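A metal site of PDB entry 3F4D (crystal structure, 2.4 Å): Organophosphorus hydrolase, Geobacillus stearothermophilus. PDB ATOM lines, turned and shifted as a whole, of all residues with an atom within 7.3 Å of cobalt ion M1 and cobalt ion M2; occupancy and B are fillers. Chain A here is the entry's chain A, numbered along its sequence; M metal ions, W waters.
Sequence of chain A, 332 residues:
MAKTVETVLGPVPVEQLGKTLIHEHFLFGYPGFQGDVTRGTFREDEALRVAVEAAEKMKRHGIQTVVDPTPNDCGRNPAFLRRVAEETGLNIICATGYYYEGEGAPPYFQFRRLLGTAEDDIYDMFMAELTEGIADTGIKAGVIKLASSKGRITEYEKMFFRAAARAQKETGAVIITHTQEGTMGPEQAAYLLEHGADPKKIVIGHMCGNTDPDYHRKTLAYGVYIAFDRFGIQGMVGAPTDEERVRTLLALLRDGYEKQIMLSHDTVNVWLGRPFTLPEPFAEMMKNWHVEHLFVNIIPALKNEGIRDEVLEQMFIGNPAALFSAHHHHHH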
ATOM      1  N   HIS A  23     -27.025  -3.774 -10.511  1.00  0.00           N
ATOM      2  CA  HIS A  23     -25.683  -4.005 -10.012  1.00  0.00           C
ATOM      3  C   HIS A  23     -25.528  -5.350  -9.355  1.00  0.00           C
ATOM      4  O   HIS A  23     -25.914  -5.525  -8.196  1.00  0.00           O
ATOM      5  CB  HIS A  23     -25.309  -2.882  -9.008  1.00  0.00           C
ATOM      6  CG  HIS A  23     -23.857  -2.856  -8.626  1.00  0.00           C
ATOM      7  ND1 HIS A  23     -23.153  -1.684  -8.472  1.00  0.00           N
ATOM      8  CD2 HIS A  23     -22.984  -3.851  -8.300  1.00  0.00           C
ATOM      9  CE1 HIS A  23     -21.916  -1.940  -8.085  1.00  0.00           C
ATOM     10  NE2 HIS A  23     -21.792  -3.248  -7.966  1.00  0.00           N
ATOM     11  N   GLU A  24     -24.966  -6.293 -10.113  1.00  0.00           N
ATOM     12  CA  GLU A  24     -24.702  -7.653  -9.670  1.00  0.00           C
ATOM     13  C   GLU A  24     -23.396  -8.147 -10.345  1.00  0.00           C
ATOM     14  O   GLU A  24     -23.053  -7.740 -11.450  1.00  0.00           O
ATOM     15  CB  GLU A  24     -25.840  -8.604 -10.050  1.00  0.00           C
ATOM     16  CG  GLU A  24     -27.245  -8.216  -9.540  1.00  0.00           C
ATOM     17  CD  GLU A  24     -27.384  -8.205  -8.013  1.00  0.00           C
ATOM     18  OE1 GLU A  24     -26.576  -8.831  -7.290  1.00  0.00           O
ATOM     19  OE2 GLU A  24     -28.330  -7.574  -7.520  1.00  0.00           O
ATOM     20  N   HIS A  25     -22.668  -9.030  -9.656  1.00  0.00           N
ATOM     21  CA  HIS A  25     -21.421  -9.564 -10.178  1.00  0.00           C
ATOM     22  C   HIS A  25     -21.494 -11.072 -10.351  1.00  0.00           C
ATOM     23  O   HIS A  25     -21.688 -11.794  -9.373  1.00  0.00           O
ATOM     24  CB  HIS A  25     -20.251  -9.279  -9.223  1.00  0.00           C
ATOM     25  CG  HIS A  25     -19.992  -7.828  -8.977  1.00  0.00           C
ATOM     26  ND1 HIS A  25     -19.212  -7.055  -9.807  1.00  0.00           N
ATOM     27  CD2 HIS A  25     -20.440  -7.001  -8.001  1.00  0.00           C
ATOM     28  CE1 HIS A  25     -19.203  -5.807  -9.360  1.00  0.00           C
ATOM     29  NE2 HIS A  25     -19.937  -5.759  -8.263  1.00  0.00           N
ATOM     30  N   PHE A  28     -16.097 -12.205  -9.432  1.00  0.00           N
ATOM     31  CA  PHE A  28     -15.431 -11.095  -8.812  1.00  0.00           C
ATOM     32  C   PHE A  28     -14.203 -11.513  -8.034  1.00  0.00           C
ATOM     33  O   PHE A  28     -14.188 -12.560  -7.358  1.00  0.00           O
ATOM     34  CB  PHE A  28     -16.384 -10.302  -7.917  1.00  0.00           C
ATOM     35  CG  PHE A  28     -15.762  -9.053  -7.369  1.00  0.00           C
ATOM     36  CD1 PHE A  28     -14.864  -9.112  -6.293  1.00  0.00           C
ATOM     37  CD2 PHE A  28     -15.978  -7.815  -7.984  1.00  0.00           C
ATOM     38  CE1 PHE A  28     -14.199  -7.998  -5.841  1.00  0.00           C
ATOM     39  CE2 PHE A  28     -15.317  -6.685  -7.548  1.00  0.00           C
ATOM     40  CZ  PHE A  28     -14.417  -6.777  -6.474  1.00  0.00           C
ATOM     41  N   PRO A  69     -21.226  -4.678 -13.358  1.00  0.00           N
ATOM     42  CA  PRO A  69     -20.177  -3.652 -13.432  1.00  0.00           C
ATOM     43  C   PRO A  69     -18.801  -4.011 -12.886  1.00  0.00           C
ATOM     44  O   PRO A  69     -18.089  -3.138 -12.413  1.00  0.00           O
ATOM     45  CB  PRO A  69     -20.802  -2.501 -12.640  1.00  0.00           C
ATOM     46  CG  PRO A  69     -21.404  -3.265 -11.470  1.00  0.00           C
ATOM     47  CD  PRO A  69     -21.970  -4.581 -12.085  1.00  0.00           C
ATOM     48  N   THR A  70     -18.439  -5.288 -12.943  1.00  0.00           N
ATOM     49  CA  THR A  70     -17.133  -5.749 -12.474  1.00  0.00           C
ATOM     50  C   THR A  70     -15.991  -5.007 -13.166  1.00  0.00           C
ATOM     51  O   THR A  70     -15.824  -5.082 -14.391  1.00  0.00           O
ATOM     52  CB  THR A  70     -16.960  -7.258 -12.719  1.00  0.00           C
ATOM     53  OG1 THR A  70     -17.980  -7.979 -12.026  1.00  0.00           O
ATOM     54  CG2 THR A  70     -15.593  -7.720 -12.215  1.00  0.00           C
ATOM     55  N   PRO A  71     -15.157  -4.298 -12.389  1.00  0.00           N
ATOM     56  CA  PRO A  71     -14.013  -3.517 -12.881  1.00  0.00           C
ATOM     57  C   PRO A  71     -12.943  -4.312 -13.666  1.00  0.00           C
ATOM     58  O   PRO A  71     -12.762  -5.493 -13.448  1.00  0.00           O
ATOM     59  CB  PRO A  71     -13.441  -2.914 -11.603  1.00  0.00           C
ATOM     60  CG  PRO A  71     -14.663  -2.797 -10.700  1.00  0.00           C
ATOM     61  CD  PRO A  71     -15.334  -4.135 -10.935  1.00  0.00           C
ATOM     62  N   TYR A  99     -11.209  -0.201 -10.277  1.00  0.00           N
ATOM     63  CA  TYR A  99     -11.739  -0.039  -8.931  1.00  0.00           C
ATOM     64  C   TYR A  99     -11.135   1.206  -8.229  1.00  0.00           C
ATOM     65  O   TYR A  99     -10.195   1.822  -8.738  1.00  0.00           O
ATOM     66  CB  TYR A  99     -11.478  -1.297  -8.103  1.00  0.00           C
ATOM     67  CG  TYR A  99     -12.623  -1.614  -7.160  1.00  0.00           C
ATOM     68  CD1 TYR A  99     -13.905  -1.147  -7.416  1.00  0.00           C
ATOM     69  CD2 TYR A  99     -12.429  -2.416  -6.018  1.00  0.00           C
ATOM     70  CE1 TYR A  99     -14.975  -1.452  -6.595  1.00  0.00           C
ATOM     71  CE2 TYR A  99     -13.508  -2.729  -5.177  1.00  0.00           C
ATOM     72  CZ  TYR A  99     -14.782  -2.240  -5.478  1.00  0.00           C
ATOM     73  OH  TYR A  99     -15.874  -2.536  -4.675  1.00  0.00           O
ATOM     74  N   TYR A 100     -11.697   1.571  -7.081  1.00  0.00           N
ATOM     75  CA  TYR A 100     -11.178   2.724  -6.366  1.00  0.00           C
ATOM     76  C   TYR A 100      -9.764   2.439  -5.839  1.00  0.00           C
ATOM     77  O   TYR A 100      -9.346   1.291  -5.714  1.00  0.00           O
ATOM     78  CB  TYR A 100     -12.143   3.133  -5.232  1.00  0.00           C
ATOM     79  CG  TYR A 100     -12.203   2.214  -4.035  1.00  0.00           C
ATOM     80  CD1 TYR A 100     -12.704   0.927  -4.151  1.00  0.00           C
ATOM     81  CD2 TYR A 100     -11.766   2.649  -2.791  1.00  0.00           C
ATOM     82  CE1 TYR A 100     -12.768   0.079  -3.044  1.00  0.00           C
ATOM     83  CE2 TYR A 100     -11.815   1.817  -1.685  1.00  0.00           C
ATOM     84  CZ  TYR A 100     -12.318   0.537  -1.813  1.00  0.00           C
ATOM     85  OH  TYR A 100     -12.355  -0.294  -0.715  1.00  0.00           O
ATOM     86  N   KCX A 145     -17.618   2.233 -15.505  1.00  0.00           N
ATOM     87  CA  KCX A 145     -17.660   2.028 -14.076  1.00  0.00           C
ATOM     88  CB  KCX A 145     -17.381   0.554 -13.740  1.00  0.00           C
ATOM     89  CG  KCX A 145     -17.277   0.280 -12.233  1.00  0.00           C
ATOM     90  CD  KCX A 145     -18.542   0.717 -11.536  1.00  0.00           C
ATOM     91  CE  KCX A 145     -18.499   0.445 -10.063  1.00  0.00           C
ATOM     92  NZ  KCX A 145     -18.398  -0.992  -9.795  1.00  0.00           N
ATOM     93  C   KCX A 145     -16.646   2.930 -13.345  1.00  0.00           C
ATOM     94  O   KCX A 145     -15.449   2.896 -13.643  1.00  0.00           O
ATOM     95  CX  KCX A 145     -18.580  -1.536  -8.604  1.00  0.00           C
ATOM     96  OQ1 KCX A 145     -18.477  -2.780  -8.430  1.00  0.00           O
ATOM     97  OQ2 KCX A 145     -18.938  -0.830  -7.624  1.00  0.00           O
ATOM     98  N   LEU A 146     -17.127   3.708 -12.386  1.00  0.00           N
ATOM     99  CA  LEU A 146     -16.261   4.583 -11.608  1.00  0.00           C
ATOM    100  C   LEU A 146     -16.395   4.288 -10.116  1.00  0.00           C
ATOM    101  O   LEU A 146     -17.413   3.756  -9.674  1.00  0.00           O
ATOM    102  CB  LEU A 146     -16.636   6.045 -11.836  1.00  0.00           C
ATOM    103  CG  LEU A 146     -16.355   6.722 -13.182  1.00  0.00           C
ATOM    104  CD1 LEU A 146     -16.958   8.140 -13.105  1.00  0.00           C
ATOM    105  CD2 LEU A 146     -14.829   6.759 -13.478  1.00  0.00           C
ATOM    106  N   ALA A 147     -15.393   4.679  -9.347  1.00  0.00           N
ATOM    107  CA  ALA A 147     -15.405   4.470  -7.890  1.00  0.00           C
ATOM    108  C   ALA A 147     -14.537   5.491  -7.143  1.00  0.00           C
ATOM    109  O   ALA A 147     -13.525   5.948  -7.644  1.00  0.00           O
ATOM    110  CB  ALA A 147     -14.940   3.053  -7.579  1.00  0.00           C
ATOM    111  N   THR A 177     -21.510   4.405 -10.674  1.00  0.00           N
ATOM    112  CA  THR A 177     -20.479   4.613  -9.670  1.00  0.00           C
ATOM    113  C   THR A 177     -20.598   3.820  -8.389  1.00  0.00           C
ATOM    114  O   THR A 177     -21.658   3.313  -8.034  1.00  0.00           O
ATOM    115  CB  THR A 177     -20.361   6.088  -9.250  1.00  0.00           C
ATOM    116  OG1 THR A 177     -21.334   6.367  -8.245  1.00  0.00           O
ATOM    117  CG2 THR A 177     -20.593   7.000 -10.424  1.00  0.00           C
ATOM    118  N   HIS A 178     -19.462   3.751  -7.698  1.00  0.00           N
ATOM    119  CA  HIS A 178     -19.323   3.077  -6.429  1.00  0.00           C
ATOM    120  C   HIS A 178     -18.884   4.144  -5.430  1.00  0.00           C
ATOM    121  O   HIS A 178     -17.920   4.859  -5.673  1.00  0.00           O
ATOM    122  CB  HIS A 178     -18.205   1.989  -6.552  1.00  0.00           C
ATOM    123  CG  HIS A 178     -17.553   1.625  -5.252  1.00  0.00           C
ATOM    124  ND1 HIS A 178     -17.550   0.340  -4.766  1.00  0.00           N
ATOM    125  CD2 HIS A 178     -16.864   2.363  -4.356  1.00  0.00           C
ATOM    126  CE1 HIS A 178     -16.897   0.304  -3.622  1.00  0.00           C
ATOM    127  NE2 HIS A 178     -16.475   1.522  -3.351  1.00  0.00           N
ATOM    128  N   THR A 179     -19.618   4.302  -4.336  1.00  0.00           N
ATOM    129  CA  THR A 179     -19.217   5.228  -3.282  1.00  0.00           C
ATOM    130  C   THR A 179     -18.836   4.324  -2.109  1.00  0.00           C
ATOM    131  O   THR A 179     -19.418   3.248  -1.902  1.00  0.00           O
ATOM    132  CB  THR A 179     -20.347   6.173  -2.816  1.00  0.00           C
ATOM    133  OG1 THR A 179     -21.490   5.401  -2.442  1.00  0.00           O
ATOM    134  CG2 THR A 179     -20.700   7.199  -3.906  1.00  0.00           C
ATOM    135  N   GLN A 180     -17.853   4.763  -1.344  1.00  0.00           N
ATOM    136  CA  GLN A 180     -17.316   3.982  -0.238  1.00  0.00           C
ATOM    137  C   GLN A 180     -17.862   4.429   1.126  1.00  0.00           C
ATOM    138  O   GLN A 180     -17.669   5.577   1.541  1.00  0.00           O
ATOM    139  CB  GLN A 180     -15.782   4.089  -0.306  1.00  0.00           C
ATOM    140  CG  GLN A 180     -14.973   3.158   0.568  1.00  0.00           C
ATOM    141  CD  GLN A 180     -15.253   1.714   0.295  1.00  0.00           C
ATOM    142  OE1 GLN A 180     -15.688   1.360  -0.789  1.00  0.00           O
ATOM    143  NE2 GLN A 180     -15.002   0.873   1.279  1.00  0.00           N
ATOM    144  N   GLY A 205     -23.788   4.931  -7.201  1.00  0.00           N
ATOM    145  CA  GLY A 205     -24.080   3.708  -6.459  1.00  0.00           C
ATOM    146  C   GLY A 205     -23.802   3.687  -4.970  1.00  0.00           C
ATOM    147  O   GLY A 205     -23.203   4.632  -4.422  1.00  0.00           O
ATOM    148  N   HIS A 206     -24.242   2.602  -4.332  1.00  0.00           N
ATOM    149  CA  HIS A 206     -24.081   2.371  -2.895  1.00  0.00           C
ATOM    150  C   HIS A 206     -24.584   3.519  -2.034  1.00  0.00           C
ATOM    151  O   HIS A 206     -24.083   3.748  -0.929  1.00  0.00           O
ATOM    152  CB  HIS A 206     -22.621   2.082  -2.546  1.00  0.00           C
ATOM    153  CG  HIS A 206     -22.024   0.982  -3.355  1.00  0.00           C
ATOM    154  ND1 HIS A 206     -22.752   0.274  -4.287  1.00  0.00           N
ATOM    155  CD2 HIS A 206     -20.763   0.517  -3.439  1.00  0.00           C
ATOM    156  CE1 HIS A 206     -21.962  -0.574  -4.922  1.00  0.00           C
ATOM    157  NE2 HIS A 206     -20.748  -0.443  -4.426  1.00  0.00           N
ATOM    158  N   ASP A 229     -28.116  -0.383  -3.869  1.00  0.00           N
ATOM    159  CA  ASP A 229     -27.673  -1.629  -4.469  1.00  0.00           C
ATOM    160  C   ASP A 229     -26.936  -2.622  -3.607  1.00  0.00           C
ATOM    161  O   ASP A 229     -26.269  -3.494  -4.138  1.00  0.00           O
ATOM    162  CB  ASP A 229     -26.803  -1.315  -5.691  1.00  0.00           C
ATOM    163  CG  ASP A 229     -25.676  -0.380  -5.351  1.00  0.00           C
ATOM    164  OD1 ASP A 229     -25.238  -0.397  -4.184  1.00  0.00           O
ATOM    165  OD2 ASP A 229     -25.223   0.369  -6.247  1.00  0.00           O
ATOM    166  N   ARG A 230     -27.046  -2.501  -2.297  1.00  0.00           N
ATOM    167  CA  ARG A 230     -26.368  -3.469  -1.464  1.00  0.00           C
ATOM    168  C   ARG A 230     -27.302  -4.200  -0.498  1.00  0.00           C
ATOM    169  O   ARG A 230     -26.874  -4.658   0.565  1.00  0.00           O
ATOM    170  CB  ARG A 230     -25.198  -2.801  -0.741  1.00  0.00           C
ATOM    171  CG  ARG A 230     -24.073  -2.423  -1.712  1.00  0.00           C
ATOM    172  CD  ARG A 230     -23.053  -1.535  -1.071  1.00  0.00           C
ATOM    173  NE  ARG A 230     -22.174  -2.286  -0.190  1.00  0.00           N
ATOM    174  CZ  ARG A 230     -21.065  -2.891  -0.600  1.00  0.00           C
ATOM    175  NH1 ARG A 230     -20.714  -2.809  -1.883  1.00  0.00           N
ATOM    176  NH2 ARG A 230     -20.318  -3.574   0.258  1.00  0.00           N
ATOM    177  N   ASP A 266     -25.846  -6.343  -5.371  1.00  0.00           N
ATOM    178  CA  ASP A 266     -24.398  -6.273  -5.502  1.00  0.00           C
ATOM    179  C   ASP A 266     -23.732  -7.633  -5.160  1.00  0.00           C
ATOM    180  O   ASP A 266     -22.595  -7.688  -4.682  1.00  0.00           O
ATOM    181  CB  ASP A 266     -23.822  -5.153  -4.632  1.00  0.00           C
ATOM    182  CG  ASP A 266     -22.345  -4.879  -4.928  1.00  0.00           C
ATOM    183  OD1 ASP A 266     -21.827  -5.398  -5.946  1.00  0.00           O
ATOM    184  OD2 ASP A 266     -21.712  -4.127  -4.141  1.00  0.00           O
ATOM    185  N   THR A 267     -24.432  -8.742  -5.442  1.00  0.00           N
ATOM    186  CA  THR A 267     -23.865 -10.046  -5.166  1.00  0.00           C
ATOM    187  C   THR A 267     -22.582 -10.360  -5.949  1.00  0.00           C
ATOM    188  O   THR A 267     -22.268  -9.741  -6.971  1.00  0.00           O
ATOM    189  CB  THR A 267     -24.853 -11.210  -5.477  1.00  0.00           C
ATOM    190  OG1 THR A 267     -25.208 -11.190  -6.878  1.00  0.00           O
ATOM    191  CG2 THR A 267     -26.118 -11.115  -4.600  1.00  0.00           C
ATOM    192  N   VAL A 268     -21.860 -11.339  -5.428  1.00  0.00           N
ATOM    193  CA  VAL A 268     -20.636 -11.846  -6.014  1.00  0.00           C
ATOM    194  C   VAL A 268     -20.969 -13.316  -6.052  1.00  0.00           C
ATOM    195  O   VAL A 268     -20.850 -14.019  -5.043  1.00  0.00           O
ATOM    196  CB  VAL A 268     -19.402 -11.659  -5.097  1.00  0.00           C
ATOM    197  CG1 VAL A 268     -18.207 -12.367  -5.696  1.00  0.00           C
ATOM    198  CG2 VAL A 268     -19.112 -10.202  -4.939  1.00  0.00           C
HETATM  199 CO    CO M   1     -18.874  -1.460  -5.417  1.00  0.00          CO
HETATM  200 CO    CO M   2     -20.099  -4.066  -7.082  1.00  0.00          CO
HETATM  201  O   HOH W   1     -19.791  -3.315  -5.214  1.00  0.00           O
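Cobalt ion M2 is bound by water W1 (2.0 Å), a ring nitrogen (NE2) of His 25 (2.1 Å), a ring nitrogen (NE2) of His 23 (2.1 Å), the side-chain carboxylate (OD1) of Asp 266 (2.5 Å) and OQ1 of KCX 145 (2.5 Å).
OH of Tyr 99 touches cobalt ion M1, 3.3 Å away. Four residues have an atom within 4 Å of cobalt ion M1: Tyr 99, KCX 145, His 178 and His 206. The nearest printed residue that does not touch cobalt ion M1 is His 23 (4.1 Å).
Within 4 Å of cobalt ion M2: His 23, His 25, KCX 145 and Asp 266. Along chain A the residues within 4 Å of cobalt ion M2 span positions 23 to 266. The nearest printed residue that does not touch cobalt ion M2 is His 206 (4.5 Å).
Water W1 is bound to cobalt ion M1, 2.1 Å away. Cobalt ion M1 is bound by OQ2 of KCX 145 (2.3 Å). Cobalt ion M1 is bound by ND1 of His 178 (2.3 Å). NE2 of His 206 binds cobalt ion M1 (2.4 Å). Cobalt ion M1 has four donor atoms within binding distance.
N of His 25 is in hydrogen-bond range of O of Thr 267 (2.8 Å). NZ of KCX 145 sits at hydrogen-bond distance from O of Pro 69, 3.4 Å away. OH of Tyr 99 sits close to ND1 of His 178 (3.3 Å). A ring nitrogen (NE2) of His 178 lies within hydrogen-bond range of the side-chain amide oxygen (OE1) of Gln 180 (2.7 Å). N of His 178 is in hydrogen-bond range of O of Leu 146. The backbone carbonyl oxygen (O) of His 206 lies within hydrogen-bond range of the side-chain hydroxyl (OG1) of Thr 179 (3.4 Å). The side-chain carboxylate of Glu 24 sits at hydrogen-bond distance from the backbone NH of Asp 266. The backbone NH (N) of Asp 266 lies close to the backbone carbonyl oxygen (O) of Asp 229.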
